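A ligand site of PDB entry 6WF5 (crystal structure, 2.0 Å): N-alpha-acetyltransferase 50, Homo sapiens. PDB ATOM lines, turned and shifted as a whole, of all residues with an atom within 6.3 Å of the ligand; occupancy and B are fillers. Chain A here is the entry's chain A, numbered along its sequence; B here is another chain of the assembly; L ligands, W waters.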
ATOM      1  N   ILE A  28      16.134 -34.538 -22.231  1.00  0.00           N
ATOM      2  CA  ILE A  28      15.590 -33.578 -23.213  1.00  0.00           C
ATOM      3  C   ILE A  28      15.985 -33.934 -24.677  1.00  0.00           C
ATOM      4  O   ILE A  28      15.122 -33.912 -25.582  1.00  0.00           O
ATOM      5  CB  ILE A  28      15.998 -32.109 -22.809  1.00  0.00           C
ATOM      6  CG1 ILE A  28      15.460 -31.758 -21.387  1.00  0.00           C
ATOM      7  CG2 ILE A  28      15.574 -31.042 -23.859  1.00  0.00           C
ATOM      8  CD1 ILE A  28      16.124 -30.506 -20.675  1.00  0.00           C
ATOM      9  N   PHE A  29      17.247 -34.285 -24.908  1.00  0.00           N
ATOM     10  CA  PHE A  29      17.734 -34.536 -26.269  1.00  0.00           C
ATOM     11  C   PHE A  29      18.102 -35.975 -26.544  1.00  0.00           C
ATOM     12  O   PHE A  29      18.806 -36.577 -25.736  1.00  0.00           O
ATOM     13  CB  PHE A  29      18.946 -33.634 -26.573  1.00  0.00           C
ATOM     14  CG  PHE A  29      18.834 -32.184 -26.172  1.00  0.00           C
ATOM     15  CD1 PHE A  29      18.278 -31.254 -27.051  1.00  0.00           C
ATOM     16  CD2 PHE A  29      19.303 -31.749 -24.937  1.00  0.00           C
ATOM     17  CE1 PHE A  29      18.197 -29.907 -26.686  1.00  0.00           C
ATOM     18  CE2 PHE A  29      19.194 -30.408 -24.567  1.00  0.00           C
ATOM     19  CZ  PHE A  29      18.643 -29.489 -25.452  1.00  0.00           C
ATOM     20  N   ILE A  76      24.406 -21.710 -30.332  1.00  0.00           N
ATOM     21  CA  ILE A  76      23.589 -22.347 -29.303  1.00  0.00           C
ATOM     22  C   ILE A  76      23.713 -23.868 -29.546  1.00  0.00           C
ATOM     23  O   ILE A  76      23.191 -24.401 -30.535  1.00  0.00           O
ATOM     24  CB  ILE A  76      22.112 -21.833 -29.281  1.00  0.00           C
ATOM     25  CG1 ILE A  76      22.059 -20.294 -29.117  1.00  0.00           C
ATOM     26  CG2 ILE A  76      21.352 -22.534 -28.139  1.00  0.00           C
ATOM     27  CD1 ILE A  76      20.597 -19.635 -29.177  1.00  0.00           C
ATOM     28  N   MET A  77      24.481 -24.543 -28.669  1.00  0.00           N
ATOM     29  CA  MET A  77      24.738 -25.991 -28.743  1.00  0.00           C
ATOM     30  C   MET A  77      23.541 -26.759 -28.285  1.00  0.00           C
ATOM     31  O   MET A  77      23.111 -27.662 -28.984  1.00  0.00           O
ATOM     32  CB  MET A  77      25.980 -26.397 -27.918  1.00  0.00           C
ATOM     33  CG  MET A  77      27.273 -25.834 -28.476  1.00  0.00           C
ATOM     34  SD  MET A  77      28.694 -26.410 -27.544  1.00  0.00           S
ATOM     35  CE  MET A  77      28.492 -25.464 -26.012  1.00  0.00           C
ATOM     36  N   THR A  78      22.971 -26.397 -27.122  1.00  0.00           N
ATOM     37  CA  THR A  78      21.763 -27.029 -26.557  1.00  0.00           C
ATOM     38  C   THR A  78      20.943 -25.967 -25.848  1.00  0.00           C
ATOM     39  O   THR A  78      21.501 -25.104 -25.183  1.00  0.00           O
ATOM     40  CB  THR A  78      22.100 -28.185 -25.586  1.00  0.00           C
ATOM     41  OG1 THR A  78      23.071 -27.748 -24.641  1.00  0.00           O
ATOM     42  CG2 THR A  78      22.577 -29.458 -26.289  1.00  0.00           C
ATOM     43  N   LEU A  79      19.616 -26.008 -26.004  1.00  0.00           N
ATOM     44  CA  LEU A  79      18.691 -25.116 -25.326  1.00  0.00           C
ATOM     45  C   LEU A  79      17.397 -25.903 -25.206  1.00  0.00           C
ATOM     46  O   LEU A  79      16.836 -26.334 -26.215  1.00  0.00           O
ATOM     47  CB  LEU A  79      18.447 -23.764 -26.051  1.00  0.00           C
ATOM     48  CG  LEU A  79      17.673 -22.657 -25.255  1.00  0.00           C
ATOM     49  CD1 LEU A  79      17.945 -21.253 -25.823  1.00  0.00           C
ATOM     50  CD2 LEU A  79      16.144 -22.879 -25.294  1.00  0.00           C
ATOM     51  N   GLY A  80      16.948 -26.116 -23.980  1.00  0.00           N
ATOM     52  CA  GLY A  80      15.740 -26.884 -23.775  1.00  0.00           C
ATOM     53  C   GLY A  80      15.335 -27.068 -22.344  1.00  0.00           C
ATOM     54  O   GLY A  80      16.153 -26.915 -21.408  1.00  0.00           O
ATOM     55  N   CYS A  81      14.086 -27.451 -22.177  1.00  0.00           N
ATOM     56  CA  CYS A  81      13.421 -27.765 -20.906  1.00  0.00           C
ATOM     57  C   CYS A  81      12.844 -29.157 -20.971  1.00  0.00           C
ATOM     58  O   CYS A  81      12.503 -29.646 -22.055  1.00  0.00           O
ATOM     59  CB  CYS A  81      12.300 -26.761 -20.626  1.00  0.00           C
ATOM     60  SG  CYS A  81      12.881 -25.073 -20.372  1.00  0.00           S
ATOM     61  N   LEU A  82      12.554 -29.712 -19.784  1.00  0.00           N
ATOM     62  CA  LEU A  82      11.873 -30.993 -19.665  1.00  0.00           C
ATOM     63  C   LEU A  82      10.450 -30.741 -20.235  1.00  0.00           C
ATOM     64  O   LEU A  82       9.889 -29.642 -20.060  1.00  0.00           O
ATOM     65  CB  LEU A  82      11.801 -31.428 -18.193  1.00  0.00           C
ATOM     66  CG  LEU A  82      13.125 -31.700 -17.421  1.00  0.00           C
ATOM     67  CD1 LEU A  82      12.817 -31.922 -15.932  1.00  0.00           C
ATOM     68  CD2 LEU A  82      13.838 -32.948 -17.940  1.00  0.00           C
ATOM     69  N   ARG A  86       7.624 -26.512 -20.726  1.00  0.00           N
ATOM     70  CA  ARG A  86       7.890 -25.760 -21.961  1.00  0.00           C
ATOM     71  C   ARG A  86       6.914 -24.569 -22.191  1.00  0.00           C
ATOM     72  O   ARG A  86       7.141 -23.750 -23.077  1.00  0.00           O
ATOM     73  CB  ARG A  86       7.935 -26.686 -23.181  1.00  0.00           C
ATOM     74  CG  ARG A  86       8.907 -27.821 -22.983  1.00  0.00           C
ATOM     75  CD  ARG A  86       9.314 -28.507 -24.254  1.00  0.00           C
ATOM     76  NE  ARG A  86      10.433 -29.390 -23.952  1.00  0.00           N
ATOM     77  CZ  ARG A  86      10.592 -30.608 -24.449  1.00  0.00           C
ATOM     78  NH1 ARG A  86       9.738 -31.078 -25.348  1.00  0.00           N
ATOM     79  NH2 ARG A  86      11.628 -31.348 -24.096  1.00  0.00           N
ATOM     80  N   ILE A  90      10.474 -20.369 -19.614  1.00  0.00           N
ATOM     81  CA  ILE A  90      11.855 -20.715 -19.267  1.00  0.00           C
ATOM     82  C   ILE A  90      12.734 -20.638 -20.540  1.00  0.00           C
ATOM     83  O   ILE A  90      13.902 -20.238 -20.464  1.00  0.00           O
ATOM     84  CB  ILE A  90      11.950 -22.095 -18.557  1.00  0.00           C
ATOM     85  CG1 ILE A  90      11.031 -22.157 -17.331  1.00  0.00           C
ATOM     86  CG2 ILE A  90      13.396 -22.366 -18.118  1.00  0.00           C
ATOM     87  CD1 ILE A  90      10.555 -23.507 -16.946  1.00  0.00           C
ATOM     88  N   GLY A  91      12.170 -21.004 -21.686  1.00  0.00           N
ATOM     89  CA  GLY A  91      12.899 -20.930 -22.943  1.00  0.00           C
ATOM     90  C   GLY A  91      13.242 -19.504 -23.322  1.00  0.00           C
ATOM     91  O   GLY A  91      14.361 -19.247 -23.757  1.00  0.00           O
ATOM     92  N   THR A  92      12.306 -18.572 -23.101  1.00  0.00           N
ATOM     93  CA  THR A  92      12.446 -17.145 -23.376  1.00  0.00           C
ATOM     94  C   THR A  92      13.497 -16.515 -22.451  1.00  0.00           C
ATOM     95  O   THR A  92      14.335 -15.732 -22.915  1.00  0.00           O
ATOM     96  CB  THR A  92      11.101 -16.430 -23.260  1.00  0.00           C
ATOM     97  OG1 THR A  92      10.174 -17.051 -24.133  1.00  0.00           O
ATOM     98  CG2 THR A  92      11.203 -14.945 -23.620  1.00  0.00           C
ATOM     99  N   MET A  94      15.957 -18.118 -20.916  1.00  0.00           N
ATOM    100  CA  MET A  94      17.237 -18.652 -21.376  1.00  0.00           C
ATOM    101  C   MET A  94      17.744 -17.969 -22.628  1.00  0.00           C
ATOM    102  O   MET A  94      18.931 -17.681 -22.687  1.00  0.00           O
ATOM    103  CB  MET A  94      17.205 -20.183 -21.594  1.00  0.00           C
ATOM    104  CG  MET A  94      16.943 -20.957 -20.311  1.00  0.00           C
ATOM    105  SD  MET A  94      17.341 -22.707 -20.437  1.00  0.00           S
ATOM    106  CE  MET A  94      16.038 -23.284 -21.528  1.00  0.00           C
ATOM    107  N   LEU A 113      21.982 -21.910 -34.593  1.00  0.00           N
ATOM    108  CA  LEU A 113      21.759 -23.225 -34.013  1.00  0.00           C
ATOM    109  C   LEU A 113      21.257 -24.214 -35.063  1.00  0.00           C
ATOM    110  O   LEU A 113      20.775 -23.811 -36.122  1.00  0.00           O
ATOM    111  CB  LEU A 113      20.707 -23.116 -32.873  1.00  0.00           C
ATOM    112  CG  LEU A 113      19.310 -22.644 -33.307  1.00  0.00           C
ATOM    113  CD1 LEU A 113      18.238 -23.566 -32.838  1.00  0.00           C
ATOM    114  CD2 LEU A 113      19.072 -21.178 -32.940  1.00  0.00           C
ATOM    115  N   HIS A 114      21.329 -25.514 -34.715  1.00  0.00           N
ATOM    116  CA  HIS A 114      20.823 -26.615 -35.517  1.00  0.00           C
ATOM    117  C   HIS A 114      19.612 -27.127 -34.821  1.00  0.00           C
ATOM    118  O   HIS A 114      19.580 -27.123 -33.586  1.00  0.00           O
ATOM    119  CB  HIS A 114      21.838 -27.760 -35.592  1.00  0.00           C
ATOM    120  CG  HIS A 114      22.966 -27.441 -36.514  1.00  0.00           C
ATOM    121  ND1 HIS A 114      24.117 -26.854 -36.042  1.00  0.00           N
ATOM    122  CD2 HIS A 114      23.057 -27.606 -37.852  1.00  0.00           C
ATOM    123  CE1 HIS A 114      24.891 -26.700 -37.095  1.00  0.00           C
ATOM    124  NE2 HIS A 114      24.301 -27.138 -38.201  1.00  0.00           N
ATOM    125  N   VAL A 115      18.616 -27.581 -35.613  1.00  0.00           N
ATOM    126  CA  VAL A 115      17.390 -28.173 -35.112  1.00  0.00           C
ATOM    127  C   VAL A 115      16.818 -29.136 -36.170  1.00  0.00           C
ATOM    128  O   VAL A 115      17.004 -28.880 -37.363  1.00  0.00           O
ATOM    129  CB  VAL A 115      16.405 -27.007 -34.724  1.00  0.00           C
ATOM    130  CG1 VAL A 115      15.745 -26.363 -35.947  1.00  0.00           C
ATOM    131  CG2 VAL A 115      15.384 -27.446 -33.686  1.00  0.00           C
ATOM    132  N   ASN A 119      10.940 -30.221 -36.015  1.00  0.00           N
ATOM    133  CA  ASN A 119      10.757 -29.570 -34.706  1.00  0.00           C
ATOM    134  C   ASN A 119      10.123 -28.176 -34.876  1.00  0.00           C
ATOM    135  O   ASN A 119      10.778 -27.153 -34.672  1.00  0.00           O
ATOM    136  CB  ASN A 119      12.118 -29.505 -33.925  1.00  0.00           C
ATOM    137  CG  ASN A 119      12.000 -29.272 -32.422  1.00  0.00           C
ATOM    138  OD1 ASN A 119      10.944 -28.918 -31.881  1.00  0.00           O
ATOM    139  ND2 ASN A 119      13.107 -29.423 -31.720  1.00  0.00           N
ATOM    140  N   SER A 121       7.784 -26.618 -33.027  1.00  0.00           N
ATOM    141  CA  SER A 121       7.673 -25.826 -31.793  1.00  0.00           C
ATOM    142  C   SER A 121       8.935 -24.964 -31.572  1.00  0.00           C
ATOM    143  O   SER A 121       8.815 -23.775 -31.295  1.00  0.00           O
ATOM    144  CB  SER A 121       7.350 -26.713 -30.588  1.00  0.00           C
ATOM    145  OG  SER A 121       8.511 -27.336 -30.059  1.00  0.00           O
ATOM    146  N   ALA A 122      10.111 -25.533 -31.806  1.00  0.00           N
ATOM    147  CA  ALA A 122      11.395 -24.838 -31.688  1.00  0.00           C
ATOM    148  C   ALA A 122      11.585 -23.848 -32.856  1.00  0.00           C
ATOM    149  O   ALA A 122      11.989 -22.698 -32.608  1.00  0.00           O
ATOM    150  CB  ALA A 122      12.533 -25.833 -31.623  1.00  0.00           C
ATOM    151  N   PHE A 125       9.297 -20.919 -32.131  1.00  0.00           N
ATOM    152  CA  PHE A 125       9.774 -20.207 -30.944  1.00  0.00           C
ATOM    153  C   PHE A 125      10.880 -19.219 -31.379  1.00  0.00           C
ATOM    154  O   PHE A 125      10.797 -18.040 -31.084  1.00  0.00           O
ATOM    155  CB  PHE A 125      10.325 -21.219 -29.917  1.00  0.00           C
ATOM    156  CG  PHE A 125      11.241 -20.633 -28.876  1.00  0.00           C
ATOM    157  CD1 PHE A 125      10.742 -19.907 -27.802  1.00  0.00           C
ATOM    158  CD2 PHE A 125      12.621 -20.848 -28.940  1.00  0.00           C
ATOM    159  CE1 PHE A 125      11.601 -19.360 -26.831  1.00  0.00           C
ATOM    160  CE2 PHE A 125      13.470 -20.322 -27.971  1.00  0.00           C
ATOM    161  CZ  PHE A 125      12.963 -19.579 -26.921  1.00  0.00           C
ATOM    162  N   TYR A 126      11.907 -19.721 -32.105  1.00  0.00           N
ATOM    163  CA  TYR A 126      13.043 -18.934 -32.601  1.00  0.00           C
ATOM    164  C   TYR A 126      12.613 -17.838 -33.561  1.00  0.00           C
ATOM    165  O   TYR A 126      13.172 -16.760 -33.485  1.00  0.00           O
ATOM    166  CB  TYR A 126      14.122 -19.809 -33.220  1.00  0.00           C
ATOM    167  CG  TYR A 126      15.015 -20.419 -32.164  1.00  0.00           C
ATOM    168  CD1 TYR A 126      15.958 -19.645 -31.490  1.00  0.00           C
ATOM    169  CD2 TYR A 126      14.908 -21.764 -31.822  1.00  0.00           C
ATOM    170  CE1 TYR A 126      16.766 -20.197 -30.490  1.00  0.00           C
ATOM    171  CE2 TYR A 126      15.719 -22.329 -30.841  1.00  0.00           C
ATOM    172  CZ  TYR A 126      16.653 -21.540 -30.192  1.00  0.00           C
ATOM    173  OH  TYR A 126      17.464 -22.122 -29.244  1.00  0.00           O
ATOM    174  C   ACE B   1      19.601 -27.370 -29.885  1.00  0.00           C
ATOM    175  O   ACE B   1      19.341 -27.744 -28.753  1.00  0.00           O
ATOM    176  CH3 ACE B   1      19.224 -25.998 -30.382  1.00  0.00           C
ATOM    177  N   MET B   2      20.241 -28.101 -30.864  1.00  0.00           N
ATOM    178  CA  MET B   2      20.680 -29.470 -30.668  1.00  0.00           C
ATOM    179  C   MET B   2      21.787 -29.740 -31.670  1.00  0.00           C
ATOM    180  O   MET B   2      21.610 -30.037 -32.838  1.00  0.00           O
ATOM    181  CB  MET B   2      19.543 -30.452 -30.863  1.00  0.00           C
ATOM    182  CG  MET B   2      20.049 -31.846 -30.455  1.00  0.00           C
ATOM    183  SD  MET B   2      18.720 -33.045 -30.308  1.00  0.00           S
ATOM    184  CE  MET B   2      18.290 -33.282 -32.046  1.00  0.00           C
HETATM  185  C1  LIG L   1      16.450 -25.886 -30.263  1.00  0.00           C
HETATM  186  C2  LIG L   1      16.117 -27.319 -29.862  1.00  0.00           C
HETATM  187  C3  LIG L   1      14.609 -28.752 -26.787  1.00  0.00           C
HETATM  188  C4  LIG L   1      12.085 -26.971 -25.579  1.00  0.00           C
HETATM  189  C5  LIG L   1      12.211 -24.529 -26.309  1.00  0.00           C
HETATM  190  S1  LIG L   1      17.915 -25.329 -29.338  1.00  0.00           S
HETATM  191  N1  LIG L   1      15.563 -27.438 -28.536  1.00  0.00           N
HETATM  192  C6  LIG L   1      14.733 -28.518 -28.265  1.00  0.00           C
HETATM  193  O1  LIG L   1      14.179 -29.224 -29.113  1.00  0.00           O
HETATM  194  C7  LIG L   1      13.164 -29.055 -26.431  1.00  0.00           C
HETATM  195  N2  LIG L   1      12.309 -27.892 -26.587  1.00  0.00           N
HETATM  196  O2  LIG L   1      12.476 -27.067 -24.419  1.00  0.00           O
HETATM  197  C8  LIG L   1      11.311 -25.748 -26.051  1.00  0.00           C
HETATM  198  O3  LIG L   1      10.622 -26.143 -27.244  1.00  0.00           O
HETATM  199  C9  LIG L   1      13.275 -24.743 -27.359  1.00  0.00           C
HETATM  200  C10 LIG L   1      12.827 -24.006 -25.027  1.00  0.00           C
HETATM  201  C11 LIG L   1      11.369 -23.382 -26.785  1.00  0.00           C
HETATM  202  O   HOH W   1      16.265 -30.775 -30.268  1.00  0.00           O
HETATM  203  O   HOH W   2      10.710 -29.212 -28.874  1.00  0.00           O
HETATM  204  O   HOH W   3      12.141 -31.736 -28.859  1.00  0.00           O
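Ile 28 touches the ligand.
Phe 29 touches the ligand (CE1 to C3, 3.8 Å).
Gly 80 touches the ligand.
CA of Gly 91 touches C10 of the ligand, at 3.7 Å.
Leu 113 touches the ligand.
Val 115 touches the ligand (CG2 to C2, 3.9 Å).
Ser 121 touches the ligand.
Phe 125 touches the ligand (CG to C11, 3.5 Å).
Met 2 of chain B touches the ligand.
Hydrophobic or aromatic side chains that line the ligand: Ile 28, Phe 29, Leu 79, Leu 113, Val 115, Phe 125 and Tyr 126.
Of the 24 residues printed, 15 come within 4 Å of the ligand.
Along chain A the residues within 4 Å of the ligand span positions 28 to 126.
The nearest printed residue that does not touch the ligand is Ala 122 (4.1 Å).
O of Cys 81 lies within hydrogen-bond range of NH2 of Arg 86, at 2.8 Å.
The side-chain hydroxyl (OG) of Ser 121 sits at hydrogen-bond distance from the side-chain amide oxygen (OD1) of Asn 119 (3.4 Å).
The backbone NH of Met 2 of chain B lies within hydrogen-bond range of the backbone carbonyl oxygen of Met 77, at 3.5 Å.
N of Leu 79 sits at hydrogen-bond distance from O of ACE 1 of chain B (3.3 Å).
The backbone carbonyl oxygen (O) of His 114 is in hydrogen-bond range of the backbone NH (N) of Met 2 of chain B, 3.0 Å away.
The side-chain amide oxygen (OD1) of Asn 119 lies close to the backbone NH (N) of Ala 122, 3.5 Å away.
ND2 of Asn 119 is in hydrogen-bond range of O1 of the ligand (2.8 Å).
A sulfur (S1) of the ligand lies close to the side-chain hydroxyl (OH) of Tyr 126.
CH3 of ACE 1 of chain B is bonded to S1 of the ligand (1.8 Å).
The backbone NH (N) of Cys 81 sits at hydrogen-bond distance from an oxygen (O2) of the ligand (2.8 Å).
The backbone carbonyl oxygen (O) of Leu 79 sits at hydrogen-bond distance from a nitrogen (N1) of the ligand (2.9 Å).
O2 of the ligand sits at hydrogen-bond distance from NE of Arg 86, at 3.1 Å.
Water W1 bridges an oxygen (O1) of the ligand (2.8 Å) and the side-chain sulfur (SD) of Met 2 of chain B (3.3 Å).
Water W2 lies within hydrogen-bond range of OD1 of Asn 119 (3.0 Å), N2 of the ligand (3.1 Å) and OG of Ser 121 (3.1 Å).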
